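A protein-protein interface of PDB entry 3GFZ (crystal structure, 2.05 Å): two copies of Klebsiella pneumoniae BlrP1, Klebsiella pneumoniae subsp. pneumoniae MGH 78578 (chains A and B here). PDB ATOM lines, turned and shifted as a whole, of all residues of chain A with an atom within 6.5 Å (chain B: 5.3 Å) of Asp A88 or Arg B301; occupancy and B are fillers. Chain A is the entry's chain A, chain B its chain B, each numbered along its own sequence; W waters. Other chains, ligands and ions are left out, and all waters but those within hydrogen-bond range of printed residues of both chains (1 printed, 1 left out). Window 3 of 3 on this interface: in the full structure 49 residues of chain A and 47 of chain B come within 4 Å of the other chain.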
ATOM      1  N   LEU A  10     -28.368   9.275 -14.846  1.00  0.00           N
ATOM      2  CA  LEU A  10     -27.837   9.780 -13.577  1.00  0.00           C
ATOM      3  C   LEU A  10     -26.856  10.943 -13.761  1.00  0.00           C
ATOM      4  O   LEU A  10     -26.031  10.936 -14.674  1.00  0.00           O
ATOM      5  CB  LEU A  10     -27.153   8.654 -12.810  1.00  0.00           C
ATOM      6  CG  LEU A  10     -26.715   8.967 -11.378  1.00  0.00           C
ATOM      7  CD1 LEU A  10     -27.929   9.180 -10.481  1.00  0.00           C
ATOM      8  CD2 LEU A  10     -25.852   7.840 -10.836  1.00  0.00           C
ATOM      9  N   THR A  11     -26.957  11.924 -12.867  1.00  0.00           N
ATOM     10  CA  THR A  11     -26.211  13.177 -12.942  1.00  0.00           C
ATOM     11  C   THR A  11     -25.796  13.597 -11.518  1.00  0.00           C
ATOM     12  O   THR A  11     -26.477  13.264 -10.552  1.00  0.00           O
ATOM     13  CB  THR A  11     -27.100  14.274 -13.577  1.00  0.00           C
ATOM     14  OG1 THR A  11     -27.460  13.894 -14.917  1.00  0.00           O
ATOM     15  CG2 THR A  11     -26.400  15.628 -13.621  1.00  0.00           C
ATOM     16  N   THR A  12     -24.676  14.309 -11.402  1.00  0.00           N
ATOM     17  CA  THR A  12     -24.222  14.866 -10.123  1.00  0.00           C
ATOM     18  C   THR A  12     -24.181  16.389 -10.249  1.00  0.00           C
ATOM     19  O   THR A  12     -23.782  16.915 -11.294  1.00  0.00           O
ATOM     20  CB  THR A  12     -22.818  14.345  -9.757  1.00  0.00           C
ATOM     21  OG1 THR A  12     -22.852  12.920  -9.656  1.00  0.00           O
ATOM     22  CG2 THR A  12     -22.318  14.925  -8.431  1.00  0.00           C
ATOM     23  N   LEU A  13     -24.575  17.077  -9.182  1.00  0.00           N
ATOM     24  CA  LEU A  13     -24.607  18.530  -9.135  1.00  0.00           C
ATOM     25  C   LEU A  13     -23.980  18.968  -7.830  1.00  0.00           C
ATOM     26  O   LEU A  13     -24.333  18.460  -6.757  1.00  0.00           O
ATOM     27  CB  LEU A  13     -26.050  19.031  -9.217  1.00  0.00           C
ATOM     28  CG  LEU A  13     -26.310  20.526  -9.485  1.00  0.00           C
ATOM     29  CD1 LEU A  13     -27.607  20.684 -10.234  1.00  0.00           C
ATOM     30  CD2 LEU A  13     -26.365  21.348  -8.231  1.00  0.00           C
ATOM     31  N   MET A  86     -19.943  21.926 -10.284  1.00  0.00           N
ATOM     32  CA  MET A  86     -19.922  20.740 -11.115  1.00  0.00           C
ATOM     33  C   MET A  86     -21.345  20.367 -11.502  1.00  0.00           C
ATOM     34  O   MET A  86     -22.269  20.485 -10.707  1.00  0.00           O
ATOM     35  CB  MET A  86     -19.255  19.593 -10.346  1.00  0.00           C
ATOM     36  CG  MET A  86     -19.095  18.280 -11.100  1.00  0.00           C
ATOM     37  SD  MET A  86     -18.465  16.975 -10.001  1.00  0.00           S
ATOM     38  CE  MET A  86     -18.462  15.598 -11.153  1.00  0.00           C
ATOM     39  N   ARG A  87     -21.511  19.947 -12.746  1.00  0.00           N
ATOM     40  CA  ARG A  87     -22.736  19.317 -13.193  1.00  0.00           C
ATOM     41  C   ARG A  87     -22.331  18.369 -14.299  1.00  0.00           C
ATOM     42  O   ARG A  87     -21.950  18.803 -15.394  1.00  0.00           O
ATOM     43  CB  ARG A  87     -23.750  20.346 -13.685  1.00  0.00           C
ATOM     44  CG  ARG A  87     -25.174  19.792 -13.764  1.00  0.00           C
ATOM     45  CD  ARG A  87     -26.143  20.807 -14.367  1.00  0.00           C
ATOM     46  NE  ARG A  87     -26.558  21.832 -13.409  1.00  0.00           N
ATOM     47  CZ  ARG A  87     -27.446  22.791 -13.661  1.00  0.00           C
ATOM     48  NH1 ARG A  87     -28.039  22.878 -14.842  1.00  0.00           N
ATOM     49  NH2 ARG A  87     -27.749  23.671 -12.725  1.00  0.00           N
ATOM     50  N   ASP A  88     -22.361  17.074 -14.007  1.00  0.00           N
ATOM     51  CA  ASP A  88     -21.864  16.102 -14.965  1.00  0.00           C
ATOM     52  C   ASP A  88     -22.666  14.828 -14.899  1.00  0.00           C
ATOM     53  O   ASP A  88     -23.313  14.550 -13.893  1.00  0.00           O
ATOM     54  CB  ASP A  88     -20.387  15.799 -14.687  1.00  0.00           C
ATOM     55  CG  ASP A  88     -19.548  15.764 -15.951  1.00  0.00           C
ATOM     56  OD1 ASP A  88     -19.973  15.153 -16.959  1.00  0.00           O
ATOM     57  OD2 ASP A  88     -18.455  16.367 -15.939  1.00  0.00           O
ATOM     58  N   TYR A  89     -22.601  14.050 -15.971  1.00  0.00           N
ATOM     59  CA  TYR A  89     -23.190  12.727 -15.974  1.00  0.00           C
ATOM     60  C   TYR A  89     -22.350  11.828 -15.067  1.00  0.00           C
ATOM     61  O   TYR A  89     -21.141  12.039 -14.915  1.00  0.00           O
ATOM     62  CB  TYR A  89     -23.287  12.175 -17.398  1.00  0.00           C
ATOM     63  CG  TYR A  89     -24.276  12.941 -18.254  1.00  0.00           C
ATOM     64  CD1 TYR A  89     -25.624  12.979 -17.915  1.00  0.00           C
ATOM     65  CD2 TYR A  89     -23.869  13.625 -19.394  1.00  0.00           C
ATOM     66  CE1 TYR A  89     -26.538  13.679 -18.676  1.00  0.00           C
ATOM     67  CE2 TYR A  89     -24.782  14.332 -20.167  1.00  0.00           C
ATOM     68  CZ  TYR A  89     -26.122  14.349 -19.799  1.00  0.00           C
ATOM     69  OH  TYR A  89     -27.046  15.038 -20.560  1.00  0.00           O
ATOM     70  N   SER A  90     -23.012  10.845 -14.461  1.00  0.00           N
ATOM     71  CA  SER A  90     -22.410  10.005 -13.435  1.00  0.00           C
ATOM     72  C   SER A  90     -22.700   8.538 -13.736  1.00  0.00           C
ATOM     73  O   SER A  90     -23.727   8.212 -14.347  1.00  0.00           O
ATOM     74  CB  SER A  90     -22.960  10.420 -12.066  1.00  0.00           C
ATOM     75  OG  SER A  90     -22.514   9.560 -11.033  1.00  0.00           O
ATOM     76  N   ALA A  91     -21.776   7.662 -13.347  1.00  0.00           N
ATOM     77  CA  ALA A  91     -21.915   6.226 -13.585  1.00  0.00           C
ATOM     78  C   ALA A  91     -22.598   5.520 -12.419  1.00  0.00           C
ATOM     79  O   ALA A  91     -23.207   4.469 -12.600  1.00  0.00           O
ATOM     80  CB  ALA A  91     -20.564   5.605 -13.836  1.00  0.00           C
ATOM     81  N   TYR A  92     -22.478   6.081 -11.220  1.00  0.00           N
ATOM     82  CA  TYR A  92     -23.071   5.470 -10.051  1.00  0.00           C
ATOM     83  C   TYR A  92     -23.296   6.503  -8.963  1.00  0.00           C
ATOM     84  O   TYR A  92     -22.724   7.592  -8.978  1.00  0.00           O
ATOM     85  CB  TYR A  92     -22.173   4.332  -9.545  1.00  0.00           C
ATOM     86  CG  TYR A  92     -20.809   4.797  -9.086  1.00  0.00           C
ATOM     87  CD1 TYR A  92     -19.757   4.936  -9.988  1.00  0.00           C
ATOM     88  CD2 TYR A  92     -20.571   5.090  -7.745  1.00  0.00           C
ATOM     89  CE1 TYR A  92     -18.505   5.370  -9.567  1.00  0.00           C
ATOM     90  CE2 TYR A  92     -19.330   5.519  -7.311  1.00  0.00           C
ATOM     91  CZ  TYR A  92     -18.300   5.657  -8.221  1.00  0.00           C
ATOM     92  OH  TYR A  92     -17.070   6.094  -7.776  1.00  0.00           O
ATOM     93  N   ARG A 132     -13.575  13.096  -8.712  1.00  0.00           N
ATOM     94  CA  ARG A 132     -13.641  14.558  -8.709  1.00  0.00           C
ATOM     95  C   ARG A 132     -14.545  15.138  -7.626  1.00  0.00           C
ATOM     96  O   ARG A 132     -14.241  16.181  -7.056  1.00  0.00           O
ATOM     97  CB  ARG A 132     -14.119  15.066 -10.061  1.00  0.00           C
ATOM     98  CG  ARG A 132     -14.153  16.567 -10.145  1.00  0.00           C
ATOM     99  CD  ARG A 132     -14.405  17.054 -11.548  1.00  0.00           C
ATOM    100  NE  ARG A 132     -14.499  18.512 -11.531  1.00  0.00           N
ATOM    101  CZ  ARG A 132     -15.276  19.249 -12.322  1.00  0.00           C
ATOM    102  NH1 ARG A 132     -16.091  18.695 -13.220  1.00  0.00           N
ATOM    103  NH2 ARG A 132     -15.249  20.570 -12.193  1.00  0.00           N
ATOM    104  N   VAL B 296     -18.772  11.376 -26.974  1.00  0.00           N
ATOM    105  CA  VAL B 296     -17.813  10.347 -26.573  1.00  0.00           C
ATOM    106  C   VAL B 296     -17.508  10.487 -25.086  1.00  0.00           C
ATOM    107  O   VAL B 296     -17.564   9.507 -24.347  1.00  0.00           O
ATOM    108  CB  VAL B 296     -16.508  10.429 -27.407  1.00  0.00           C
ATOM    109  CG1 VAL B 296     -15.378   9.611 -26.769  1.00  0.00           C
ATOM    110  CG2 VAL B 296     -16.769   9.956 -28.834  1.00  0.00           C
ATOM    111  N   LEU B 297     -17.185  11.706 -24.659  1.00  0.00           N
ATOM    112  CA  LEU B 297     -16.920  11.998 -23.248  1.00  0.00           C
ATOM    113  C   LEU B 297     -18.125  11.628 -22.394  1.00  0.00           C
ATOM    114  O   LEU B 297     -17.969  11.026 -21.335  1.00  0.00           O
ATOM    115  CB  LEU B 297     -16.559  13.481 -23.067  1.00  0.00           C
ATOM    116  CG  LEU B 297     -16.069  14.044 -21.718  1.00  0.00           C
ATOM    117  CD1 LEU B 297     -17.206  14.508 -20.826  1.00  0.00           C
ATOM    118  CD2 LEU B 297     -15.188  13.065 -20.964  1.00  0.00           C
ATOM    119  N   LYS B 298     -19.319  11.975 -22.873  1.00  0.00           N
ATOM    120  CA  LYS B 298     -20.568  11.623 -22.201  1.00  0.00           C
ATOM    121  C   LYS B 298     -20.697  10.117 -22.004  1.00  0.00           C
ATOM    122  O   LYS B 298     -21.015   9.657 -20.910  1.00  0.00           O
ATOM    123  CB  LYS B 298     -21.768  12.142 -22.997  1.00  0.00           C
ATOM    124  CG  LYS B 298     -23.121  11.679 -22.475  1.00  0.00           C
ATOM    125  CD  LYS B 298     -24.248  12.459 -23.121  1.00  0.00           C
ATOM    126  CE  LYS B 298     -25.599  11.884 -22.754  1.00  0.00           C
ATOM    127  NZ  LYS B 298     -25.864  10.598 -23.467  1.00  0.00           N
ATOM    128  N   ALA B 299     -20.457   9.360 -23.069  1.00  0.00           N
ATOM    129  CA  ALA B 299     -20.535   7.905 -23.007  1.00  0.00           C
ATOM    130  C   ALA B 299     -19.496   7.335 -22.043  1.00  0.00           C
ATOM    131  O   ALA B 299     -19.799   6.438 -21.255  1.00  0.00           O
ATOM    132  CB  ALA B 299     -20.357   7.311 -24.394  1.00  0.00           C
ATOM    133  N   LEU B 300     -18.278   7.865 -22.103  1.00  0.00           N
ATOM    134  CA  LEU B 300     -17.210   7.443 -21.196  1.00  0.00           C
ATOM    135  C   LEU B 300     -17.539   7.732 -19.730  1.00  0.00           C
ATOM    136  O   LEU B 300     -17.246   6.912 -18.860  1.00  0.00           O
ATOM    137  CB  LEU B 300     -15.887   8.123 -21.555  1.00  0.00           C
ATOM    138  CG  LEU B 300     -15.177   7.676 -22.835  1.00  0.00           C
ATOM    139  CD1 LEU B 300     -13.960   8.569 -23.067  1.00  0.00           C
ATOM    140  CD2 LEU B 300     -14.761   6.207 -22.781  1.00  0.00           C
ATOM    141  N   ARG B 301     -18.145   8.893 -19.476  1.00  0.00           N
ATOM    142  CA  ARG B 301     -18.566   9.298 -18.131  1.00  0.00           C
ATOM    143  C   ARG B 301     -19.617   8.367 -17.548  1.00  0.00           C
ATOM    144  O   ARG B 301     -19.475   7.893 -16.427  1.00  0.00           O
ATOM    145  CB  ARG B 301     -19.135  10.722 -18.145  1.00  0.00           C
ATOM    146  CG  ARG B 301     -18.086  11.799 -18.117  1.00  0.00           C
ATOM    147  CD  ARG B 301     -17.658  12.123 -16.692  1.00  0.00           C
ATOM    148  NE  ARG B 301     -16.243  12.478 -16.627  1.00  0.00           N
ATOM    149  CZ  ARG B 301     -15.722  13.666 -16.940  1.00  0.00           C
ATOM    150  NH1 ARG B 301     -16.480  14.681 -17.354  1.00  0.00           N
ATOM    151  NH2 ARG B 301     -14.412  13.840 -16.833  1.00  0.00           N
ATOM    152  N   VAL B 302     -20.670   8.116 -18.313  1.00  0.00           N
ATOM    153  CA  VAL B 302     -21.772   7.274 -17.855  1.00  0.00           C
ATOM    154  C   VAL B 302     -21.291   5.843 -17.605  1.00  0.00           C
ATOM    155  O   VAL B 302     -21.739   5.197 -16.664  1.00  0.00           O
ATOM    156  CB  VAL B 302     -22.953   7.302 -18.857  1.00  0.00           C
ATOM    157  CG1 VAL B 302     -24.033   6.274 -18.490  1.00  0.00           C
ATOM    158  CG2 VAL B 302     -23.565   8.700 -18.912  1.00  0.00           C
ATOM    159  N   ALA B 303     -20.372   5.360 -18.438  1.00  0.00           N
ATOM    160  CA  ALA B 303     -19.799   4.022 -18.272  1.00  0.00           C
ATOM    161  C   ALA B 303     -18.878   3.913 -17.050  1.00  0.00           C
ATOM    162  O   ALA B 303     -18.670   2.818 -16.532  1.00  0.00           O
ATOM    163  CB  ALA B 303     -19.046   3.616 -19.524  1.00  0.00           C
ATOM    164  N   GLY B 304     -18.313   5.038 -16.618  1.00  0.00           N
ATOM    165  CA  GLY B 304     -17.529   5.111 -15.381  1.00  0.00           C
ATOM    166  C   GLY B 304     -16.030   5.248 -15.578  1.00  0.00           C
ATOM    167  O   GLY B 304     -15.285   5.316 -14.600  1.00  0.00           O
ATOM    168  N   MET B 305     -15.578   5.292 -16.830  1.00  0.00           N
ATOM    169  CA  MET B 305     -14.160   5.481 -17.118  1.00  0.00           C
ATOM    170  C   MET B 305     -13.774   6.939 -16.877  1.00  0.00           C
ATOM    171  O   MET B 305     -14.634   7.821 -16.858  1.00  0.00           O
ATOM    172  CB  MET B 305     -13.824   5.066 -18.558  1.00  0.00           C
ATOM    173  CG  MET B 305     -13.727   3.556 -18.758  1.00  0.00           C
ATOM    174  SD  MET B 305     -13.420   3.071 -20.469  1.00  0.00           S
ATOM    175  CE  MET B 305     -15.076   3.221 -21.135  1.00  0.00           C
ATOM    176  N   LEU B 307     -11.040  10.373 -17.716  1.00  0.00           N
ATOM    177  CA  LEU B 307     -10.426  11.040 -18.860  1.00  0.00           C
ATOM    178  C   LEU B 307      -9.333  11.988 -18.396  1.00  0.00           C
ATOM    179  O   LEU B 307      -9.531  12.722 -17.424  1.00  0.00           O
ATOM    180  CB  LEU B 307     -11.482  11.836 -19.629  1.00  0.00           C
ATOM    181  CG  LEU B 307     -10.976  12.502 -20.915  1.00  0.00           C
ATOM    182  CD1 LEU B 307     -11.282  11.629 -22.136  1.00  0.00           C
ATOM    183  CD2 LEU B 307     -11.572  13.895 -21.070  1.00  0.00           C
ATOM    184  N   GLN B 326     -14.741  19.375 -17.965  1.00  0.00           N
ATOM    185  CA  GLN B 326     -13.623  19.249 -17.054  1.00  0.00           C
ATOM    186  C   GLN B 326     -13.127  17.804 -17.109  1.00  0.00           C
ATOM    187  O   GLN B 326     -13.915  16.888 -16.925  1.00  0.00           O
ATOM    188  CB  GLN B 326     -14.059  19.629 -15.634  1.00  0.00           C
ATOM    189  CG  GLN B 326     -14.427  21.115 -15.452  1.00  0.00           C
ATOM    190  CD  GLN B 326     -15.870  21.461 -15.840  1.00  0.00           C
ATOM    191  OE1 GLN B 326     -16.790  20.658 -15.686  1.00  0.00           O
ATOM    192  NE2 GLN B 326     -16.068  22.675 -16.331  1.00  0.00           N
ATOM    193  N   PRO B 327     -11.828  17.593 -17.380  1.00  0.00           N
ATOM    194  CA  PRO B 327     -11.296  16.240 -17.311  1.00  0.00           C
ATOM    195  C   PRO B 327     -11.085  15.836 -15.861  1.00  0.00           C
ATOM    196  O   PRO B 327     -11.163  16.676 -14.969  1.00  0.00           O
ATOM    197  CB  PRO B 327      -9.949  16.368 -18.016  1.00  0.00           C
ATOM    198  CG  PRO B 327      -9.540  17.757 -17.748  1.00  0.00           C
ATOM    199  CD  PRO B 327     -10.782  18.563 -17.754  1.00  0.00           C
ATOM    200  N   ASP B 328     -10.818  14.560 -15.632  1.00  0.00           N
ATOM    201  CA  ASP B 328     -10.498  14.088 -14.294  1.00  0.00           C
ATOM    202  C   ASP B 328      -9.065  14.438 -13.934  1.00  0.00           C
ATOM    203  O   ASP B 328      -8.752  14.643 -12.762  1.00  0.00           O
ATOM    204  CB  ASP B 328     -10.738  12.588 -14.197  1.00  0.00           C
ATOM    205  CG  ASP B 328     -12.209  12.237 -14.340  1.00  0.00           C
ATOM    206  OD1 ASP B 328     -13.011  12.670 -13.483  1.00  0.00           O
ATOM    207  OD2 ASP B 328     -12.561  11.559 -15.326  1.00  0.00           O
HETATM  208  O   HOH W   1     -17.249  18.067 -17.786  1.00  0.00           O
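The side-chain carboxylate (OD2) of Asp A88 lies within salt-bridge range of the guanidinium group (NH1) of Arg B301. OE1 of Gln B326 is in hydrogen-bond range of NH1 of Arg A132, 3.2 Å away.
The backbone NH (N) of Thr A12 sits at hydrogen-bond distance from the backbone carbonyl oxygen (O) of Asp A88, at 2.8 Å. NH2 of Arg B301 is in hydrogen-bond range of O of Gln B326 (3.1 Å). The side-chain carboxylate (OD2) of Asp B328 lies within salt-bridge range of the guanidinium group (NH2) of Arg B301.
Among the printed residues, merely in contact across the chains: Tyr A89 with Lys B298 (3.5 Å), Tyr A89 with Arg B301 (3.9 Å), Tyr A89 with Val B302 (3.8 Å), Ala A91 with Arg B301 (3.6 Å), Ala A91 with Val B302 (3.1 Å) and Ala A91 with Gly B304 (3.4 Å).
Asp A88 touches just one residue of chain B: Arg B301. Printed residues of chain B within 4 Å of Ala A91: Arg B301, Val B302 and Gly B304. Leu B297 touches none of the printed residues of chain A. Of the printed residues of chain A, Lys B298 touches Tyr A89. Of chain A, only Asp A88, Tyr A89 and Ala A91 come within 4 Å of Arg B301. Of the printed residues of chain A, Val B302 touches Tyr A89 and Ala A91. The nearest residue of chain A that does not touch Arg B301 is Ser A90 (4.2 Å).
Of the 14 printed residues of chain B, 5 touch a printed residue of chain A. Hydrophobic or aromatic side chains of chain B that line the printed part of chain A: Val B302. Of the 12 printed residues of chain A, 4 touch a printed residue of chain B. Hydrophobic or aromatic side chains of chain A within 4 Å of the printed part of chain B: Tyr A89 and Ala A91. Among the printed residues, 8 pairs touch across the chains. Among the printed residues, Asp or Glu carboxylates within 4 Å of a Lys or Arg side-chain nitrogen of the other chain: Asp A88 with Arg B301.
No position is printed for both chains.
Water W1 lies within hydrogen-bond range of OD2 of Asp A88 (2.8 Å), N of Gln B326 (2.8 Å) and NH1 of Arg B301 (3.5 Å).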
